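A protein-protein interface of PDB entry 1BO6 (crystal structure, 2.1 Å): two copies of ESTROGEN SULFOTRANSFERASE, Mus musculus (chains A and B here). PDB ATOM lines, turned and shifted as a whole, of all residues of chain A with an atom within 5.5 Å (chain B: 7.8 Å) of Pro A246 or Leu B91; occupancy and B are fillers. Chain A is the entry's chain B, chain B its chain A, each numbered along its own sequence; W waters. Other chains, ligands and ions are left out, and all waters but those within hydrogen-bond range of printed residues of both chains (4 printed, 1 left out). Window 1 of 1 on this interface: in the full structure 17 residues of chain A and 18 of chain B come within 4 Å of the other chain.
The guanidinium group (NH1) of Arg B25 lies within salt-bridge range of the side-chain carboxylate (OE2) of Glu A248, 3.5 Å away. The backbone carbonyl oxygen (O) of Asp B90 is in hydrogen-bond range of the side-chain amide nitrogen (ND2) of Asn A79. The backbone NH (N) of Asp B90 sits at hydrogen-bond distance from the backbone carbonyl oxygen (O) of Met A244, at 3.2 Å. The side-chain sulfur of Met A244 lies close to the side-chain carboxylate of Glu B89.
NE of Arg B87 is in hydrogen-bond range of O of Glu B89 (2.8 Å).
Phe A78 touches Asp B90 (CE1 to O, 3.7 Å). Leu A91 touches Ile B92. Leu A91 touches Pro B246 (CD2 to CG, 3.3 Å). CG1 of Ile A92 touches CD1 of Leu B91 (3.8 Å). N of Leu B91 touches O of Met A244 (3.7 Å). Asn B88 touches Pro A246 (OD1 to CG, 3.7 Å). CG of Pro A246 touches CD2 of Leu B91 (3.2 Å). CB of Glu A248 touches O of Glu B248, 3.5 Å away. OE2 of Glu A248 touches CE of Met B249, at 3.1 Å. Met A249 touches Glu B248 (CE to OE2, 3.2 Å).
Of chain B, only Asn B88 (3.7 Å) and Leu B91 (3.2 Å) come within 4 Å of Pro A246. Of the printed residues of chain A, Leu B91 touches Ile A92, Met A244 and Pro A246. Of the printed residues of chain A, Glu B89 touches Met A244. Printed residues of chain B within 4 Å of Leu A91: Ile B92 (3.8 Å) and Pro B246 (3.3 Å). Printed residues of chain B within 4 Å of Ile A92: Leu B91 (3.8 Å). Of the printed residues of chain B, Met A244 touches Glu B89, Asp B90 and Leu B91. Printed residues of chain A within 4 Å of Met B249: Glu A248 (3.1 Å). Asn A251 touches none of the printed residues of chain B. The nearest printed residue of chain A that does not touch Ile B92 is Pro A246 (5.4 Å).
Of the 13 printed residues of chain A, 8 touch a printed residue of chain B. Hydrophobic or aromatic side chains of chain A that line the printed part of chain B: Phe A78, Leu A91, Ile A92, Met A244, Pro A246 and Met A249. Of the 13 printed residues of chain B, 9 touch a printed residue of chain A. Printed residues of chain B that touch a printed residue of chain A: Arg B25, Asn B88, Glu B89, Asp B90, Leu B91, Ile B92, Pro B246, Glu B248 and Met B249. Among the printed residues, 14 pairs touch across the chains.
Leu A91 touches Ile B92, and with the chains exchanged Ile A92 touches Leu B91. Leu A91 touches Pro B246, and with the chains exchanged Pro A246 touches Leu B91. Glu B248 touches its own counterpart, Glu A248. Glu A248 touches Met B249, and with the chains exchanged Met A249 touches Glu B248. Positions printed for both chains: 91, 92, 246, 248 and 249.
Water W4 lies within hydrogen-bond range of the side-chain carboxylate of Glu A248 (2.6 Å), the guanidinium group of Arg B25 (2.9 Å) and the side-chain amide oxygen of Asn B88 (3.4 Å). Water W1 bridges the backbone carbonyl oxygen (O) of Asp B90 (2.8 Å) and the side-chain amide nitrogen (ND2) of Asn A79 (3.2 Å). Water W3 bridges the side-chain carboxylate (OE2) of Glu B248 and the backbone carbonyl oxygen (O) of Met A249. Water W2 bridges OE2 of Glu A248 (3.0 Å) and O of Met B249 (3.0 Å).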
ATOM      1  N   PHE A  78     -18.905  19.152  20.006  1.00  0.00           N
ATOM      2  CA  PHE A  78     -19.660  18.317  20.929  1.00  0.00           C
ATOM      3  C   PHE A  78     -20.958  17.794  20.322  1.00  0.00           C
ATOM      4  O   PHE A  78     -21.653  16.989  20.938  1.00  0.00           O
ATOM      5  CB  PHE A  78     -19.940  19.056  22.250  1.00  0.00           C
ATOM      6  CG  PHE A  78     -20.528  20.436  22.085  1.00  0.00           C
ATOM      7  CD1 PHE A  78     -21.892  20.607  21.849  1.00  0.00           C
ATOM      8  CD2 PHE A  78     -19.731  21.568  22.237  1.00  0.00           C
ATOM      9  CE1 PHE A  78     -22.454  21.887  21.773  1.00  0.00           C
ATOM     10  CE2 PHE A  78     -20.282  22.851  22.164  1.00  0.00           C
ATOM     11  CZ  PHE A  78     -21.645  23.009  21.934  1.00  0.00           C
ATOM     12  N   ASN A  79     -21.276  18.251  19.112  1.00  0.00           N
ATOM     13  CA  ASN A  79     -22.473  17.807  18.403  1.00  0.00           C
ATOM     14  C   ASN A  79     -22.006  16.847  17.321  1.00  0.00           C
ATOM     15  O   ASN A  79     -22.659  15.841  17.037  1.00  0.00           O
ATOM     16  CB  ASN A  79     -23.200  18.990  17.751  1.00  0.00           C
ATOM     17  CG  ASN A  79     -23.984  19.826  18.754  1.00  0.00           C
ATOM     18  OD1 ASN A  79     -24.275  19.379  19.866  1.00  0.00           O
ATOM     19  ND2 ASN A  79     -24.331  21.052  18.361  1.00  0.00           N
ATOM     20  N   LEU A  91     -31.867  18.565  29.232  1.00  0.00           N
ATOM     21  CA  LEU A  91     -31.257  19.588  28.394  1.00  0.00           C
ATOM     22  C   LEU A  91     -30.088  19.015  27.595  1.00  0.00           C
ATOM     23  O   LEU A  91     -29.972  19.257  26.395  1.00  0.00           O
ATOM     24  CB  LEU A  91     -30.768  20.762  29.243  1.00  0.00           C
ATOM     25  CG  LEU A  91     -30.075  21.841  28.402  1.00  0.00           C
ATOM     26  CD1 LEU A  91     -31.115  22.580  27.567  1.00  0.00           C
ATOM     27  CD2 LEU A  91     -29.310  22.804  29.295  1.00  0.00           C
ATOM     28  N   ILE A  92     -29.223  18.258  28.266  1.00  0.00           N
ATOM     29  CA  ILE A  92     -28.061  17.647  27.610  1.00  0.00           C
ATOM     30  C   ILE A  92     -28.088  16.125  27.745  1.00  0.00           C
ATOM     31  O   ILE A  92     -28.220  15.593  28.845  1.00  0.00           O
ATOM     32  CB  ILE A  92     -26.731  18.171  28.217  1.00  0.00           C
ATOM     33  CG1 ILE A  92     -26.661  19.691  28.092  1.00  0.00           C
ATOM     34  CG2 ILE A  92     -25.534  17.533  27.505  1.00  0.00           C
ATOM     35  CD1 ILE A  92     -25.643  20.328  29.014  1.00  0.00           C
ATOM     36  N   THR A 243     -16.716  27.893  22.502  1.00  0.00           N
ATOM     37  CA  THR A 243     -17.372  29.177  22.709  1.00  0.00           C
ATOM     38  C   THR A 243     -18.830  29.021  22.257  1.00  0.00           C
ATOM     39  O   THR A 243     -19.642  29.932  22.410  1.00  0.00           O
ATOM     40  CB  THR A 243     -16.683  30.306  21.903  1.00  0.00           C
ATOM     41  OG1 THR A 243     -16.528  29.901  20.535  1.00  0.00           O
ATOM     42  CG2 THR A 243     -15.312  30.629  22.500  1.00  0.00           C
ATOM     43  N   MET A 244     -19.142  27.851  21.694  1.00  0.00           N
ATOM     44  CA  MET A 244     -20.497  27.528  21.236  1.00  0.00           C
ATOM     45  C   MET A 244     -21.242  26.925  22.420  1.00  0.00           C
ATOM     46  O   MET A 244     -22.383  26.473  22.295  1.00  0.00           O
ATOM     47  CB  MET A 244     -20.461  26.498  20.100  1.00  0.00           C
ATOM     48  CG  MET A 244     -20.020  27.041  18.750  1.00  0.00           C
ATOM     49  SD  MET A 244     -21.163  28.244  18.051  1.00  0.00           S
ATOM     50  CE  MET A 244     -20.470  29.791  18.673  1.00  0.00           C
ATOM     51  N   MET A 245     -20.577  26.921  23.570  1.00  0.00           N
ATOM     52  CA  MET A 245     -21.135  26.372  24.799  1.00  0.00           C
ATOM     53  C   MET A 245     -21.380  27.488  25.823  1.00  0.00           C
ATOM     54  O   MET A 245     -20.445  28.171  26.237  1.00  0.00           O
ATOM     55  CB  MET A 245     -20.175  25.325  25.374  1.00  0.00           C
ATOM     56  CG  MET A 245     -20.571  24.781  26.735  1.00  0.00           C
ATOM     57  SD  MET A 245     -21.863  23.537  26.621  1.00  0.00           S
ATOM     58  CE  MET A 245     -21.169  22.432  25.386  1.00  0.00           C
ATOM     59  N   PRO A 246     -22.647  27.679  26.239  1.00  0.00           N
ATOM     60  CA  PRO A 246     -23.092  28.689  27.208  1.00  0.00           C
ATOM     61  C   PRO A 246     -22.143  28.971  28.363  1.00  0.00           C
ATOM     62  O   PRO A 246     -21.686  28.059  29.045  1.00  0.00           O
ATOM     63  CB  PRO A 246     -24.431  28.147  27.699  1.00  0.00           C
ATOM     64  CG  PRO A 246     -24.970  27.424  26.515  1.00  0.00           C
ATOM     65  CD  PRO A 246     -23.780  26.875  25.745  1.00  0.00           C
ATOM     66  N   GLU A 247     -21.874  30.252  28.586  1.00  0.00           N
ATOM     67  CA  GLU A 247     -20.989  30.696  29.651  1.00  0.00           C
ATOM     68  C   GLU A 247     -21.517  30.304  31.027  1.00  0.00           C
ATOM     69  O   GLU A 247     -20.755  30.206  31.990  1.00  0.00           O
ATOM     70  CB  GLU A 247     -20.820  32.214  29.566  1.00  0.00           C
ATOM     71  CG  GLU A 247     -20.424  32.891  30.867  1.00  0.00           C
ATOM     72  CD  GLU A 247     -19.616  34.157  30.634  1.00  0.00           C
ATOM     73  OE1 GLU A 247     -18.850  34.204  29.645  1.00  0.00           O
ATOM     74  OE2 GLU A 247     -19.750  35.105  31.440  1.00  0.00           O
ATOM     75  N   GLU A 248     -22.823  30.087  31.125  1.00  0.00           N
ATOM     76  CA  GLU A 248     -23.420  29.700  32.400  1.00  0.00           C
ATOM     77  C   GLU A 248     -22.927  28.308  32.793  1.00  0.00           C
ATOM     78  O   GLU A 248     -22.973  27.931  33.960  1.00  0.00           O
ATOM     79  CB  GLU A 248     -24.951  29.699  32.301  1.00  0.00           C
ATOM     80  CG  GLU A 248     -25.566  31.056  32.001  1.00  0.00           C
ATOM     81  CD  GLU A 248     -26.049  31.159  30.571  1.00  0.00           C
ATOM     82  OE1 GLU A 248     -25.200  31.110  29.656  1.00  0.00           O
ATOM     83  OE2 GLU A 248     -27.273  31.281  30.358  1.00  0.00           O
ATOM     84  N   MET A 249     -22.460  27.554  31.804  1.00  0.00           N
ATOM     85  CA  MET A 249     -21.947  26.205  32.030  1.00  0.00           C
ATOM     86  C   MET A 249     -20.415  26.217  32.083  1.00  0.00           C
ATOM     87  O   MET A 249     -19.806  25.809  33.075  1.00  0.00           O
ATOM     88  CB  MET A 249     -22.400  25.268  30.905  1.00  0.00           C
ATOM     89  CG  MET A 249     -23.757  25.602  30.314  1.00  0.00           C
ATOM     90  SD  MET A 249     -24.994  24.359  30.711  1.00  0.00           S
ATOM     91  CE  MET A 249     -25.122  24.568  32.465  1.00  0.00           C
ATOM     92  N   MET A 250     -19.810  26.683  30.994  1.00  0.00           N
ATOM     93  CA  MET A 250     -18.363  26.769  30.860  1.00  0.00           C
ATOM     94  C   MET A 250     -17.957  28.228  30.822  1.00  0.00           C
ATOM     95  O   MET A 250     -18.049  28.867  29.778  1.00  0.00           O
ATOM     96  CB  MET A 250     -17.918  26.115  29.555  1.00  0.00           C
ATOM     97  CG  MET A 250     -17.458  24.682  29.682  1.00  0.00           C
ATOM     98  SD  MET A 250     -16.806  24.067  28.119  1.00  0.00           S
ATOM     99  CE  MET A 250     -15.554  25.285  27.789  1.00  0.00           C
ATOM    100  N   ASN A 251     -17.501  28.753  31.949  1.00  0.00           N
ATOM    101  CA  ASN A 251     -17.088  30.147  32.001  1.00  0.00           C
ATOM    102  C   ASN A 251     -15.638  30.332  31.559  1.00  0.00           C
ATOM    103  O   ASN A 251     -14.717  30.299  32.377  1.00  0.00           O
ATOM    104  CB  ASN A 251     -17.262  30.692  33.416  1.00  0.00           C
ATOM    105  CG  ASN A 251     -17.038  32.178  33.483  1.00  0.00           C
ATOM    106  OD1 ASN A 251     -16.861  32.830  32.454  1.00  0.00           O
ATOM    107  ND2 ASN A 251     -17.044  32.726  34.692  1.00  0.00           N
ATOM    108  N   ARG B  25     -29.171  36.779  22.047  1.00  0.00           N
ATOM    109  CA  ARG B  25     -28.880  35.411  21.653  1.00  0.00           C
ATOM    110  C   ARG B  25     -29.955  34.855  20.716  1.00  0.00           C
ATOM    111  O   ARG B  25     -29.685  33.954  19.909  1.00  0.00           O
ATOM    112  CB  ARG B  25     -28.754  34.526  22.895  1.00  0.00           C
ATOM    113  CG  ARG B  25     -27.521  34.828  23.735  1.00  0.00           C
ATOM    114  CD  ARG B  25     -27.536  34.047  25.038  1.00  0.00           C
ATOM    115  NE  ARG B  25     -28.571  34.544  25.935  1.00  0.00           N
ATOM    116  CZ  ARG B  25     -28.588  34.336  27.248  1.00  0.00           C
ATOM    117  NH1 ARG B  25     -27.622  33.636  27.826  1.00  0.00           N
ATOM    118  NH2 ARG B  25     -29.570  34.836  27.988  1.00  0.00           N
ATOM    119  N   ARG B  87     -32.622  30.105  21.493  1.00  0.00           N
ATOM    120  CA  ARG B  87     -31.349  29.727  20.932  1.00  0.00           C
ATOM    121  C   ARG B  87     -30.221  30.200  21.830  1.00  0.00           C
ATOM    122  O   ARG B  87     -30.230  31.333  22.310  1.00  0.00           O
ATOM    123  CB  ARG B  87     -31.224  30.344  19.540  1.00  0.00           C
ATOM    124  CG  ARG B  87     -29.847  30.252  18.916  1.00  0.00           C
ATOM    125  CD  ARG B  87     -29.638  28.902  18.250  1.00  0.00           C
ATOM    126  NE  ARG B  87     -28.399  28.864  17.484  1.00  0.00           N
ATOM    127  CZ  ARG B  87     -28.346  28.952  16.160  1.00  0.00           C
ATOM    128  NH1 ARG B  87     -29.460  29.082  15.459  1.00  0.00           N
ATOM    129  NH2 ARG B  87     -27.176  28.903  15.533  1.00  0.00           N
ATOM    130  N   ASN B  88     -29.270  29.308  22.086  1.00  0.00           N
ATOM    131  CA  ASN B  88     -28.097  29.639  22.890  1.00  0.00           C
ATOM    132  C   ASN B  88     -26.906  28.971  22.216  1.00  0.00           C
ATOM    133  O   ASN B  88     -26.417  27.939  22.666  1.00  0.00           O
ATOM    134  CB  ASN B  88     -28.241  29.136  24.326  1.00  0.00           C
ATOM    135  CG  ASN B  88     -27.391  29.934  25.304  1.00  0.00           C
ATOM    136  OD1 ASN B  88     -26.324  30.443  24.944  1.00  0.00           O
ATOM    137  ND2 ASN B  88     -27.864  30.051  26.546  1.00  0.00           N
ATOM    138  N   GLU B  89     -26.473  29.576  21.116  1.00  0.00           N
ATOM    139  CA  GLU B  89     -25.366  29.074  20.326  1.00  0.00           C
ATOM    140  C   GLU B  89     -25.659  27.649  19.859  1.00  0.00           C
ATOM    141  O   GLU B  89     -26.697  27.404  19.238  1.00  0.00           O
ATOM    142  CB  GLU B  89     -24.062  29.142  21.126  1.00  0.00           C
ATOM    143  CG  GLU B  89     -23.460  30.545  21.196  1.00  0.00           C
ATOM    144  CD  GLU B  89     -23.382  31.236  19.839  1.00  0.00           C
ATOM    145  OE1 GLU B  89     -23.347  30.545  18.798  1.00  0.00           O
ATOM    146  OE2 GLU B  89     -23.350  32.484  19.812  1.00  0.00           O
ATOM    147  N   ASP B  90     -24.764  26.710  20.157  1.00  0.00           N
ATOM    148  CA  ASP B  90     -24.955  25.328  19.721  1.00  0.00           C
ATOM    149  C   ASP B  90     -25.487  24.390  20.792  1.00  0.00           C
ATOM    150  O   ASP B  90     -25.705  23.216  20.528  1.00  0.00           O
ATOM    151  CB  ASP B  90     -23.645  24.772  19.155  1.00  0.00           C
ATOM    152  CG  ASP B  90     -23.367  25.267  17.748  1.00  0.00           C
ATOM    153  OD1 ASP B  90     -24.298  25.818  17.124  1.00  0.00           O
ATOM    154  OD2 ASP B  90     -22.225  25.110  17.263  1.00  0.00           O
ATOM    155  N   LEU B  91     -25.692  24.899  22.001  1.00  0.00           N
ATOM    156  CA  LEU B  91     -26.216  24.065  23.074  1.00  0.00           C
ATOM    157  C   LEU B  91     -27.738  23.974  22.996  1.00  0.00           C
ATOM    158  O   LEU B  91     -28.303  22.892  23.107  1.00  0.00           O
ATOM    159  CB  LEU B  91     -25.810  24.612  24.443  1.00  0.00           C
ATOM    160  CG  LEU B  91     -26.391  23.784  25.595  1.00  0.00           C
ATOM    161  CD1 LEU B  91     -25.681  22.445  25.659  1.00  0.00           C
ATOM    162  CD2 LEU B  91     -26.251  24.525  26.906  1.00  0.00           C
ATOM    163  N   ILE B  92     -28.398  25.116  22.808  1.00  0.00           N
ATOM    164  CA  ILE B  92     -29.862  25.157  22.711  1.00  0.00           C
ATOM    165  C   ILE B  92     -30.303  25.750  21.371  1.00  0.00           C
ATOM    166  O   ILE B  92     -29.845  26.823  20.969  1.00  0.00           O
ATOM    167  CB  ILE B  92     -30.482  26.005  23.854  1.00  0.00           C
ATOM    168  CG1 ILE B  92     -30.093  25.422  25.214  1.00  0.00           C
ATOM    169  CG2 ILE B  92     -31.998  26.034  23.729  1.00  0.00           C
ATOM    170  CD1 ILE B  92     -30.266  26.402  26.367  1.00  0.00           C
ATOM    171  N   ASN B  93     -31.188  25.044  20.678  1.00  0.00           N
ATOM    172  CA  ASN B  93     -31.675  25.509  19.389  1.00  0.00           C
ATOM    173  C   ASN B  93     -33.083  24.974  19.094  1.00  0.00           C
ATOM    174  O   ASN B  93     -33.246  23.830  18.672  1.00  0.00           O
ATOM    175  CB  ASN B  93     -30.702  25.078  18.293  1.00  0.00           C
ATOM    176  CG  ASN B  93     -30.983  25.746  16.967  1.00  0.00           C
ATOM    177  OD1 ASN B  93     -30.073  25.980  16.176  1.00  0.00           O
ATOM    178  ND2 ASN B  93     -32.249  26.050  16.710  1.00  0.00           N
ATOM    179  N   GLY B  94     -34.096  25.814  19.312  1.00  0.00           N
ATOM    180  CA  GLY B  94     -35.467  25.405  19.071  1.00  0.00           C
ATOM    181  C   GLY B  94     -35.781  25.073  17.627  1.00  0.00           C
ATOM    182  O   GLY B  94     -36.523  24.130  17.356  1.00  0.00           O
ATOM    183  N   GLN B  97     -34.638  21.704  16.802  1.00  0.00           N
ATOM    184  CA  GLN B  97     -35.563  20.764  17.416  1.00  0.00           C
ATOM    185  C   GLN B  97     -36.799  20.571  16.553  1.00  0.00           C
ATOM    186  O   GLN B  97     -37.257  19.445  16.346  1.00  0.00           O
ATOM    187  CB  GLN B  97     -36.015  21.288  18.770  1.00  0.00           C
ATOM    188  CG  GLN B  97     -35.105  20.983  19.920  1.00  0.00           C
ATOM    189  CD  GLN B  97     -35.692  21.453  21.227  1.00  0.00           C
ATOM    190  OE1 GLN B  97     -36.371  20.699  21.925  1.00  0.00           O
ATOM    191  NE2 GLN B  97     -35.442  22.712  21.569  1.00  0.00           N
ATOM    192  N   PRO B 246     -31.328  22.731  33.795  1.00  0.00           N
ATOM    193  CA  PRO B 246     -30.155  23.091  34.603  1.00  0.00           C
ATOM    194  C   PRO B 246     -30.277  24.363  35.426  1.00  0.00           C
ATOM    195  O   PRO B 246     -30.651  25.418  34.913  1.00  0.00           O
ATOM    196  CB  PRO B 246     -29.035  23.194  33.578  1.00  0.00           C
ATOM    197  CG  PRO B 246     -29.412  22.199  32.547  1.00  0.00           C
ATOM    198  CD  PRO B 246     -30.927  22.148  32.502  1.00  0.00           C
ATOM    199  N   GLU B 248     -28.025  26.175  36.441  1.00  0.00           N
ATOM    200  CA  GLU B 248     -27.082  27.189  35.981  1.00  0.00           C
ATOM    201  C   GLU B 248     -27.780  28.155  35.029  1.00  0.00           C
ATOM    202  O   GLU B 248     -27.313  29.274  34.810  1.00  0.00           O
ATOM    203  CB  GLU B 248     -25.893  26.538  35.269  1.00  0.00           C
ATOM    204  CG  GLU B 248     -25.062  25.622  36.147  1.00  0.00           C
ATOM    205  CD  GLU B 248     -25.312  24.160  35.839  1.00  0.00           C
ATOM    206  OE1 GLU B 248     -26.445  23.689  36.078  1.00  0.00           O
ATOM    207  OE2 GLU B 248     -24.382  23.482  35.350  1.00  0.00           O
ATOM    208  N   MET B 249     -28.902  27.708  34.468  1.00  0.00           N
ATOM    209  CA  MET B 249     -29.691  28.518  33.544  1.00  0.00           C
ATOM    210  C   MET B 249     -30.892  29.124  34.267  1.00  0.00           C
ATOM    211  O   MET B 249     -31.052  30.345  34.324  1.00  0.00           O
ATOM    212  CB  MET B 249     -30.192  27.658  32.382  1.00  0.00           C
ATOM    213  CG  MET B 249     -29.257  26.535  31.976  1.00  0.00           C
ATOM    214  SD  MET B 249     -28.563  26.819  30.353  1.00  0.00           S
ATOM    215  CE  MET B 249     -27.525  28.225  30.698  1.00  0.00           C
HETATM  216  O   HOH W   1     -27.316  22.262  18.493  1.00  0.00           O
HETATM  217  O   HOH W   2     -29.652  31.871  32.105  1.00  0.00           O
HETATM  218  O   HOH W   3     -21.661  24.072  34.869  1.00  0.00           O
HETATM  219  O   HOH W   4     -24.996  32.389  27.409  1.00  0.00           O
